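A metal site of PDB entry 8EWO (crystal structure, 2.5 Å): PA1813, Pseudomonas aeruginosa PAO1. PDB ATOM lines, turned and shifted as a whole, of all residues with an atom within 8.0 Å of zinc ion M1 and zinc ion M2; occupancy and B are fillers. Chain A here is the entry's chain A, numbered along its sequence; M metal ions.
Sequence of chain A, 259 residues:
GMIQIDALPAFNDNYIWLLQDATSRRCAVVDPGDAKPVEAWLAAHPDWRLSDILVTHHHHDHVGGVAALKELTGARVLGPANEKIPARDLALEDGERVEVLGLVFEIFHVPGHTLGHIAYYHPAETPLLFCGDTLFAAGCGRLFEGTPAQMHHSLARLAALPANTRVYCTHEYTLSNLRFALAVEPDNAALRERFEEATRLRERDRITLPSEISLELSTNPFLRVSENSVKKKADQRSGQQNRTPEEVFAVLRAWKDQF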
ATOM      1  N   ASP A  13      -3.452 -11.592 -38.513  1.00  0.00           N
ATOM      2  CA  ASP A  13      -3.556 -12.969 -38.056  1.00  0.00           C
ATOM      3  C   ASP A  13      -3.833 -13.075 -36.557  1.00  0.00           C
ATOM      4  O   ASP A  13      -3.568 -14.118 -35.955  1.00  0.00           O
ATOM      5  CB  ASP A  13      -2.271 -13.740 -38.392  1.00  0.00           C
ATOM      6  CG  ASP A  13      -1.026 -12.889 -38.227  1.00  0.00           C
ATOM      7  OD1 ASP A  13      -0.996 -12.030 -37.309  1.00  0.00           O
ATOM      8  OD2 ASP A  13      -0.067 -13.066 -39.008  1.00  0.00           O
ATOM      9  N   ASN A  14      -4.365 -12.020 -35.941  1.00  0.00           N
ATOM     10  CA  ASN A  14      -4.603 -12.010 -34.507  1.00  0.00           C
ATOM     11  C   ASN A  14      -5.982 -12.563 -34.183  1.00  0.00           C
ATOM     12  O   ASN A  14      -6.934 -12.427 -34.965  1.00  0.00           O
ATOM     13  CB  ASN A  14      -4.479 -10.585 -33.943  1.00  0.00           C
ATOM     14  CG  ASN A  14      -3.062 -10.260 -33.528  1.00  0.00           C
ATOM     15  OD1 ASN A  14      -2.710 -10.319 -32.347  1.00  0.00           O
ATOM     16  ND2 ASN A  14      -2.222  -9.905 -34.494  1.00  0.00           N
ATOM     17  N   ASP A  31      -6.195 -10.367 -24.606  1.00  0.00           N
ATOM     18  CA  ASP A  31      -5.325  -9.613 -25.506  1.00  0.00           C
ATOM     19  C   ASP A  31      -6.101  -8.863 -26.577  1.00  0.00           C
ATOM     20  O   ASP A  31      -6.003  -9.192 -27.765  1.00  0.00           O
ATOM     21  CB  ASP A  31      -4.312 -10.553 -26.160  1.00  0.00           C
ATOM     22  CG  ASP A  31      -3.254 -11.057 -25.185  1.00  0.00           C
ATOM     23  OD1 ASP A  31      -2.980 -10.356 -24.194  1.00  0.00           O
ATOM     24  OD2 ASP A  31      -2.707 -12.148 -25.418  1.00  0.00           O
ATOM     25  N   THR A  56      -1.587 -11.046 -21.852  1.00  0.00           N
ATOM     26  CA  THR A  56      -0.457 -11.965 -21.715  1.00  0.00           C
ATOM     27  C   THR A  56       0.885 -11.243 -21.691  1.00  0.00           C
ATOM     28  O   THR A  56       1.682 -11.464 -20.770  1.00  0.00           O
ATOM     29  CB  THR A  56      -0.473 -13.001 -22.840  1.00  0.00           C
ATOM     30  OG1 THR A  56      -0.345 -12.346 -24.108  1.00  0.00           O
ATOM     31  CG2 THR A  56      -1.766 -13.802 -22.809  1.00  0.00           C
ATOM     32  N   HIS A  57       1.162 -10.391 -22.681  1.00  0.00           N
ATOM     33  CA  HIS A  57       2.390  -9.596 -22.694  1.00  0.00           C
ATOM     34  C   HIS A  57       2.096  -8.224 -23.280  1.00  0.00           C
ATOM     35  O   HIS A  57       0.992  -7.945 -23.765  1.00  0.00           O
ATOM     36  CB  HIS A  57       3.523 -10.304 -23.453  1.00  0.00           C
ATOM     37  CG  HIS A  57       3.235 -10.545 -24.910  1.00  0.00           C
ATOM     38  ND1 HIS A  57       2.183 -11.321 -25.339  1.00  0.00           N
ATOM     39  CD2 HIS A  57       3.875 -10.126 -26.022  1.00  0.00           C
ATOM     40  CE1 HIS A  57       2.189 -11.360 -26.665  1.00  0.00           C
ATOM     41  NE2 HIS A  57       3.197 -10.645 -27.096  1.00  0.00           N
ATOM     42  N   HIS A  58       3.105  -7.362 -23.244  1.00  0.00           N
ATOM     43  CA  HIS A  58       2.958  -5.929 -23.470  1.00  0.00           C
ATOM     44  C   HIS A  58       2.946  -5.524 -24.948  1.00  0.00           C
ATOM     45  O   HIS A  58       2.968  -4.324 -25.235  1.00  0.00           O
ATOM     46  CB  HIS A  58       4.079  -5.167 -22.754  1.00  0.00           C
ATOM     47  CG  HIS A  58       5.430  -5.373 -23.364  1.00  0.00           C
ATOM     48  ND1 HIS A  58       6.012  -4.458 -24.215  1.00  0.00           N
ATOM     49  CD2 HIS A  58       6.318  -6.393 -23.260  1.00  0.00           C
ATOM     50  CE1 HIS A  58       7.194  -4.903 -24.600  1.00  0.00           C
ATOM     51  NE2 HIS A  58       7.407  -6.077 -24.031  1.00  0.00           N
ATOM     52  N   HIS A  59       2.921  -6.475 -25.877  1.00  0.00           N
ATOM     53  CA  HIS A  59       3.081  -6.122 -27.279  1.00  0.00           C
ATOM     54  C   HIS A  59       1.846  -5.402 -27.817  1.00  0.00           C
ATOM     55  O   HIS A  59       0.729  -5.583 -27.323  1.00  0.00           O
ATOM     56  CB  HIS A  59       3.380  -7.364 -28.113  1.00  0.00           C
ATOM     57  CG  HIS A  59       4.834  -7.711 -28.156  1.00  0.00           C
ATOM     58  ND1 HIS A  59       5.319  -8.851 -28.753  1.00  0.00           N
ATOM     59  CD2 HIS A  59       5.919  -7.056 -27.663  1.00  0.00           C
ATOM     60  CE1 HIS A  59       6.637  -8.888 -28.634  1.00  0.00           C
ATOM     61  NE2 HIS A  59       7.029  -7.812 -27.981  1.00  0.00           N
ATOM     62  N   HIS A  60       2.072  -4.577 -28.846  1.00  0.00           N
ATOM     63  CA  HIS A  60       1.037  -3.665 -29.331  1.00  0.00           C
ATOM     64  C   HIS A  60      -0.210  -4.415 -29.771  1.00  0.00           C
ATOM     65  O   HIS A  60      -1.335  -3.972 -29.497  1.00  0.00           O
ATOM     66  CB  HIS A  60       1.585  -2.836 -30.492  1.00  0.00           C
ATOM     67  CG  HIS A  60       1.789  -3.618 -31.753  1.00  0.00           C
ATOM     68  ND1 HIS A  60       2.897  -4.415 -31.958  1.00  0.00           N
ATOM     69  CD2 HIS A  60       1.006  -3.752 -32.842  1.00  0.00           C
ATOM     70  CE1 HIS A  60       2.798  -4.995 -33.140  1.00  0.00           C
ATOM     71  NE2 HIS A  60       1.658  -4.614 -33.706  1.00  0.00           N
ATOM     72  N   ASP A  61      -0.043  -5.542 -30.458  1.00  0.00           N
ATOM     73  CA  ASP A  61      -1.195  -6.263 -30.990  1.00  0.00           C
ATOM     74  C   ASP A  61      -1.978  -7.004 -29.909  1.00  0.00           C
ATOM     75  O   ASP A  61      -2.902  -7.761 -30.246  1.00  0.00           O
ATOM     76  CB  ASP A  61      -0.749  -7.242 -32.074  1.00  0.00           C
ATOM     77  CG  ASP A  61       0.418  -8.101 -31.644  1.00  0.00           C
ATOM     78  OD1 ASP A  61       1.421  -7.539 -31.145  1.00  0.00           O
ATOM     79  OD2 ASP A  61       0.335  -9.335 -31.779  1.00  0.00           O
ATOM     80  N   HIS A  62      -1.644  -6.802 -28.634  1.00  0.00           N
ATOM     81  CA  HIS A  62      -2.360  -7.407 -27.528  1.00  0.00           C
ATOM     82  C   HIS A  62      -2.952  -6.400 -26.556  1.00  0.00           C
ATOM     83  O   HIS A  62      -3.884  -6.749 -25.828  1.00  0.00           O
ATOM     84  CB  HIS A  62      -1.453  -8.362 -26.749  1.00  0.00           C
ATOM     85  CG  HIS A  62      -0.840  -9.433 -27.593  1.00  0.00           C
ATOM     86  ND1 HIS A  62      -1.255 -10.744 -27.541  1.00  0.00           N
ATOM     87  CD2 HIS A  62       0.150  -9.389 -28.515  1.00  0.00           C
ATOM     88  CE1 HIS A  62      -0.549 -11.467 -28.401  1.00  0.00           C
ATOM     89  NE2 HIS A  62       0.310 -10.667 -29.002  1.00  0.00           N
ATOM     90  N   HIS A 113       9.400 -15.079 -25.242  1.00  0.00           N
ATOM     91  CA  HIS A 113       8.950 -14.079 -26.211  1.00  0.00           C
ATOM     92  C   HIS A 113       9.178 -12.677 -25.670  1.00  0.00           C
ATOM     93  O   HIS A 113       9.756 -11.818 -26.349  1.00  0.00           O
ATOM     94  CB  HIS A 113       7.472 -14.316 -26.535  1.00  0.00           C
ATOM     95  CG  HIS A 113       6.930 -13.393 -27.577  1.00  0.00           C
ATOM     96  ND1 HIS A 113       7.219 -13.521 -28.915  1.00  0.00           N
ATOM     97  CD2 HIS A 113       6.082 -12.343 -27.477  1.00  0.00           C
ATOM     98  CE1 HIS A 113       6.587 -12.585 -29.597  1.00  0.00           C
ATOM     99  NE2 HIS A 113       5.887 -11.852 -28.745  1.00  0.00           N
ATOM    100  N   THR A 114       8.730 -12.422 -24.441  1.00  0.00           N
ATOM    101  CA  THR A 114       9.079 -11.238 -23.681  1.00  0.00           C
ATOM    102  C   THR A 114       9.524 -11.685 -22.291  1.00  0.00           C
ATOM    103  O   THR A 114       9.323 -12.827 -21.894  1.00  0.00           O
ATOM    104  CB  THR A 114       7.910 -10.249 -23.576  1.00  0.00           C
ATOM    105  OG1 THR A 114       6.832 -10.845 -22.851  1.00  0.00           O
ATOM    106  CG2 THR A 114       7.433  -9.829 -24.963  1.00  0.00           C
ATOM    107  N   HIS A 117       6.205 -12.139 -20.014  1.00  0.00           N
ATOM    108  CA  HIS A 117       5.069 -12.872 -20.549  1.00  0.00           C
ATOM    109  C   HIS A 117       4.499 -13.854 -19.529  1.00  0.00           C
ATOM    110  O   HIS A 117       5.241 -14.544 -18.825  1.00  0.00           O
ATOM    111  CB  HIS A 117       5.491 -13.628 -21.817  1.00  0.00           C
ATOM    112  CG  HIS A 117       4.355 -14.004 -22.719  1.00  0.00           C
ATOM    113  ND1 HIS A 117       3.259 -14.702 -22.286  1.00  0.00           N
ATOM    114  CD2 HIS A 117       4.171 -13.791 -24.043  1.00  0.00           C
ATOM    115  CE1 HIS A 117       2.428 -14.898 -23.299  1.00  0.00           C
ATOM    116  NE2 HIS A 117       2.965 -14.355 -24.374  1.00  0.00           N
ATOM    117  N   GLY A 132      -0.872 -16.773 -25.222  1.00  0.00           N
ATOM    118  CA  GLY A 132      -0.466 -15.590 -25.983  1.00  0.00           C
ATOM    119  C   GLY A 132       0.473 -15.928 -27.123  1.00  0.00           C
ATOM    120  O   GLY A 132       0.111 -16.635 -28.077  1.00  0.00           O
ATOM    121  N   ASP A 133       1.701 -15.405 -27.037  1.00  0.00           N
ATOM    122  CA  ASP A 133       2.715 -15.595 -28.077  1.00  0.00           C
ATOM    123  C   ASP A 133       3.829 -16.541 -27.648  1.00  0.00           C
ATOM    124  O   ASP A 133       4.854 -16.615 -28.331  1.00  0.00           O
ATOM    125  CB  ASP A 133       3.319 -14.249 -28.473  1.00  0.00           C
ATOM    126  CG  ASP A 133       2.393 -13.434 -29.349  1.00  0.00           C
ATOM    127  OD1 ASP A 133       1.253 -13.890 -29.601  1.00  0.00           O
ATOM    128  OD2 ASP A 133       2.798 -12.345 -29.804  1.00  0.00           O
ATOM    129  N   THR A 134       3.661 -17.254 -26.529  1.00  0.00           N
ATOM    130  CA  THR A 134       4.711 -18.158 -26.072  1.00  0.00           C
ATOM    131  C   THR A 134       4.688 -19.471 -26.862  1.00  0.00           C
ATOM    132  O   THR A 134       5.624 -19.772 -27.602  1.00  0.00           O
ATOM    133  CB  THR A 134       4.568 -18.423 -24.566  1.00  0.00           C
ATOM    134  OG1 THR A 134       4.699 -17.186 -23.853  1.00  0.00           O
ATOM    135  CG2 THR A 134       5.633 -19.396 -24.084  1.00  0.00           C
ATOM    136  N   PHE A 136       2.809 -21.620 -29.780  1.00  0.00           N
ATOM    137  CA  PHE A 136       1.926 -21.555 -30.937  1.00  0.00           C
ATOM    138  C   PHE A 136       1.557 -22.960 -31.390  1.00  0.00           C
ATOM    139  O   PHE A 136       2.171 -23.952 -30.980  1.00  0.00           O
ATOM    140  CB  PHE A 136       2.588 -20.779 -32.086  1.00  0.00           C
ATOM    141  CG  PHE A 136       2.578 -19.292 -31.893  1.00  0.00           C
ATOM    142  CD1 PHE A 136       1.428 -18.634 -31.528  1.00  0.00           C
ATOM    143  CD2 PHE A 136       3.734 -18.556 -32.108  1.00  0.00           C
ATOM    144  CE1 PHE A 136       1.420 -17.258 -31.362  1.00  0.00           C
ATOM    145  CE2 PHE A 136       3.734 -17.186 -31.944  1.00  0.00           C
ATOM    146  CZ  PHE A 136       2.577 -16.537 -31.570  1.00  0.00           C
ATOM    147  N   GLY A 141       6.908 -18.510 -30.156  1.00  0.00           N
ATOM    148  CA  GLY A 141       7.180 -17.123 -30.461  1.00  0.00           C
ATOM    149  C   GLY A 141       8.650 -16.843 -30.662  1.00  0.00           C
ATOM    150  O   GLY A 141       9.527 -17.600 -30.248  1.00  0.00           O
ATOM    151  N   ARG A 142       8.928 -15.717 -31.319  1.00  0.00           N
ATOM    152  CA  ARG A 142      10.292 -15.278 -31.516  1.00  0.00           C
ATOM    153  C   ARG A 142      10.830 -14.668 -30.229  1.00  0.00           C
ATOM    154  O   ARG A 142      10.085 -14.125 -29.404  1.00  0.00           O
ATOM    155  CB  ARG A 142      10.378 -14.249 -32.655  1.00  0.00           C
ATOM    156  CG  ARG A 142       9.958 -14.805 -34.007  1.00  0.00           C
ATOM    157  CD  ARG A 142       9.877 -13.700 -35.041  1.00  0.00           C
ATOM    158  NE  ARG A 142      11.193 -13.191 -35.408  1.00  0.00           N
ATOM    159  CZ  ARG A 142      11.866 -13.544 -36.488  1.00  0.00           C
ATOM    160  NH1 ARG A 142      11.376 -14.406 -37.361  1.00  0.00           N
ATOM    161  NH2 ARG A 142      13.062 -13.006 -36.709  1.00  0.00           N
ATOM    162  N   PHE A 144      12.035 -12.023 -28.800  1.00  0.00           N
ATOM    163  CA  PHE A 144      12.180 -10.573 -28.827  1.00  0.00           C
ATOM    164  C   PHE A 144      12.974 -10.073 -27.630  1.00  0.00           C
ATOM    165  O   PHE A 144      13.729  -9.098 -27.761  1.00  0.00           O
ATOM    166  CB  PHE A 144      10.812  -9.905 -28.878  1.00  0.00           C
ATOM    167  CG  PHE A 144      10.208  -9.844 -30.253  1.00  0.00           C
ATOM    168  CD1 PHE A 144      10.695  -8.970 -31.210  1.00  0.00           C
ATOM    169  CD2 PHE A 144       9.133 -10.655 -30.578  1.00  0.00           C
ATOM    170  CE1 PHE A 144      10.135  -8.921 -32.473  1.00  0.00           C
ATOM    171  CE2 PHE A 144       8.567 -10.614 -31.843  1.00  0.00           C
ATOM    172  CZ  PHE A 144       9.068  -9.740 -32.789  1.00  0.00           C
ATOM    173  N   THR A 170      -2.426 -16.818 -29.773  1.00  0.00           N
ATOM    174  CA  THR A 170      -3.018 -15.602 -30.314  1.00  0.00           C
ATOM    175  C   THR A 170      -3.085 -15.584 -31.835  1.00  0.00           C
ATOM    176  O   THR A 170      -4.085 -15.132 -32.399  1.00  0.00           O
ATOM    177  CB  THR A 170      -2.227 -14.379 -29.828  1.00  0.00           C
ATOM    178  OG1 THR A 170      -2.139 -14.402 -28.400  1.00  0.00           O
ATOM    179  CG2 THR A 170      -2.905 -13.092 -30.283  1.00  0.00           C
ATOM    180  N   HIS A 171      -2.056 -16.076 -32.515  1.00  0.00           N
ATOM    181  CA  HIS A 171      -1.884 -15.805 -33.936  1.00  0.00           C
ATOM    182  C   HIS A 171      -2.230 -17.016 -34.795  1.00  0.00           C
ATOM    183  O   HIS A 171      -2.097 -18.166 -34.377  1.00  0.00           O
ATOM    184  CB  HIS A 171      -0.449 -15.368 -34.234  1.00  0.00           C
ATOM    185  CG  HIS A 171      -0.092 -14.033 -33.674  1.00  0.00           C
ATOM    186  ND1 HIS A 171      -0.358 -12.847 -34.324  1.00  0.00           N
ATOM    187  CD2 HIS A 171       0.524 -13.684 -32.509  1.00  0.00           C
ATOM    188  CE1 HIS A 171       0.073 -11.835 -33.593  1.00  0.00           C
ATOM    189  NE2 HIS A 171       0.612 -12.319 -32.487  1.00  0.00           N
ATOM    190  N   TYR A 173      -0.732 -18.691 -37.080  1.00  0.00           N
ATOM    191  CA  TYR A 173       0.572 -19.058 -37.628  1.00  0.00           C
ATOM    192  C   TYR A 173       0.678 -20.532 -37.999  1.00  0.00           C
ATOM    193  O   TYR A 173       1.759 -20.978 -38.378  1.00  0.00           O
ATOM    194  CB  TYR A 173       1.677 -18.711 -36.621  1.00  0.00           C
ATOM    195  CG  TYR A 173       1.939 -17.237 -36.402  1.00  0.00           C
ATOM    196  CD1 TYR A 173       1.603 -16.303 -37.362  1.00  0.00           C
ATOM    197  CD2 TYR A 173       2.571 -16.795 -35.245  1.00  0.00           C
ATOM    198  CE1 TYR A 173       1.846 -14.951 -37.162  1.00  0.00           C
ATOM    199  CE2 TYR A 173       2.822 -15.451 -35.036  1.00  0.00           C
ATOM    200  CZ  TYR A 173       2.460 -14.537 -35.992  1.00  0.00           C
ATOM    201  OH  TYR A 173       2.719 -13.197 -35.795  1.00  0.00           O
HETATM  202 ZN    ZN M   1       1.579 -10.972 -30.894  1.00  0.00          ZN
HETATM  203 ZN    ZN M   2       3.989 -10.647 -29.159  1.00  0.00          ZN
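Zinc ion M1 is bound by the side-chain carboxylate (OD2) of Asp 133, at 2.1 Å. Zinc ion M1 is bound by the side-chain carboxylate (OD2) of Asp 61 (2.2 Å). A ring nitrogen (NE2) of His 62 is bound to zinc ion M1. A ring nitrogen (NE2) of His 171 is bound to zinc ion M1, at 2.3 Å. Zinc ion M1 has four donor atoms within binding distance.
Within 4 Å of zinc ion M2: His 57, His 59, His 62, His 113 and Asp 133. The nearest printed residue that does not touch zinc ion M2 is Asp 61 (4.5 Å).
Along chain A the residues within 4 Å of zinc ion M1 span positions 61 to 171.
A ring nitrogen (NE2) of His 117 lies within hydrogen-bond range of the backbone NH of Asp 133, 3.1 Å away. N of Gly 141 sits close to O of Asp 133, 3.3 Å away. NE2 of His 117 is in hydrogen-bond range of ND1 of His 57 (3.3 Å). OG1 of Thr 56 is in hydrogen-bond range of ND1 of His 57, at 3.0 Å. The side-chain amide oxygen of Asn 14 sits close to the backbone carbonyl oxygen of Asp 61, at 3.3 Å. A ring nitrogen (ND1) of His 113 lies within hydrogen-bond range of the backbone carbonyl oxygen of Arg 142, at 3.0 Å. ND1 of His 171 sits at hydrogen-bond distance from OH of Tyr 173 (3.4 Å). ND1 of His 171 sits at hydrogen-bond distance from OD1 of Asp 13, at 3.2 Å.
Zinc ion M2 is bound by the side-chain carboxylate of Asp 133 (2.2 Å), a ring nitrogen (NE2) of His 57 (2.2 Å), a ring nitrogen (ND1) of His 59 (2.3 Å) and a ring nitrogen (NE2) of His 113 (2.3 Å). Zinc ion M2 has four donor atoms within binding distance.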
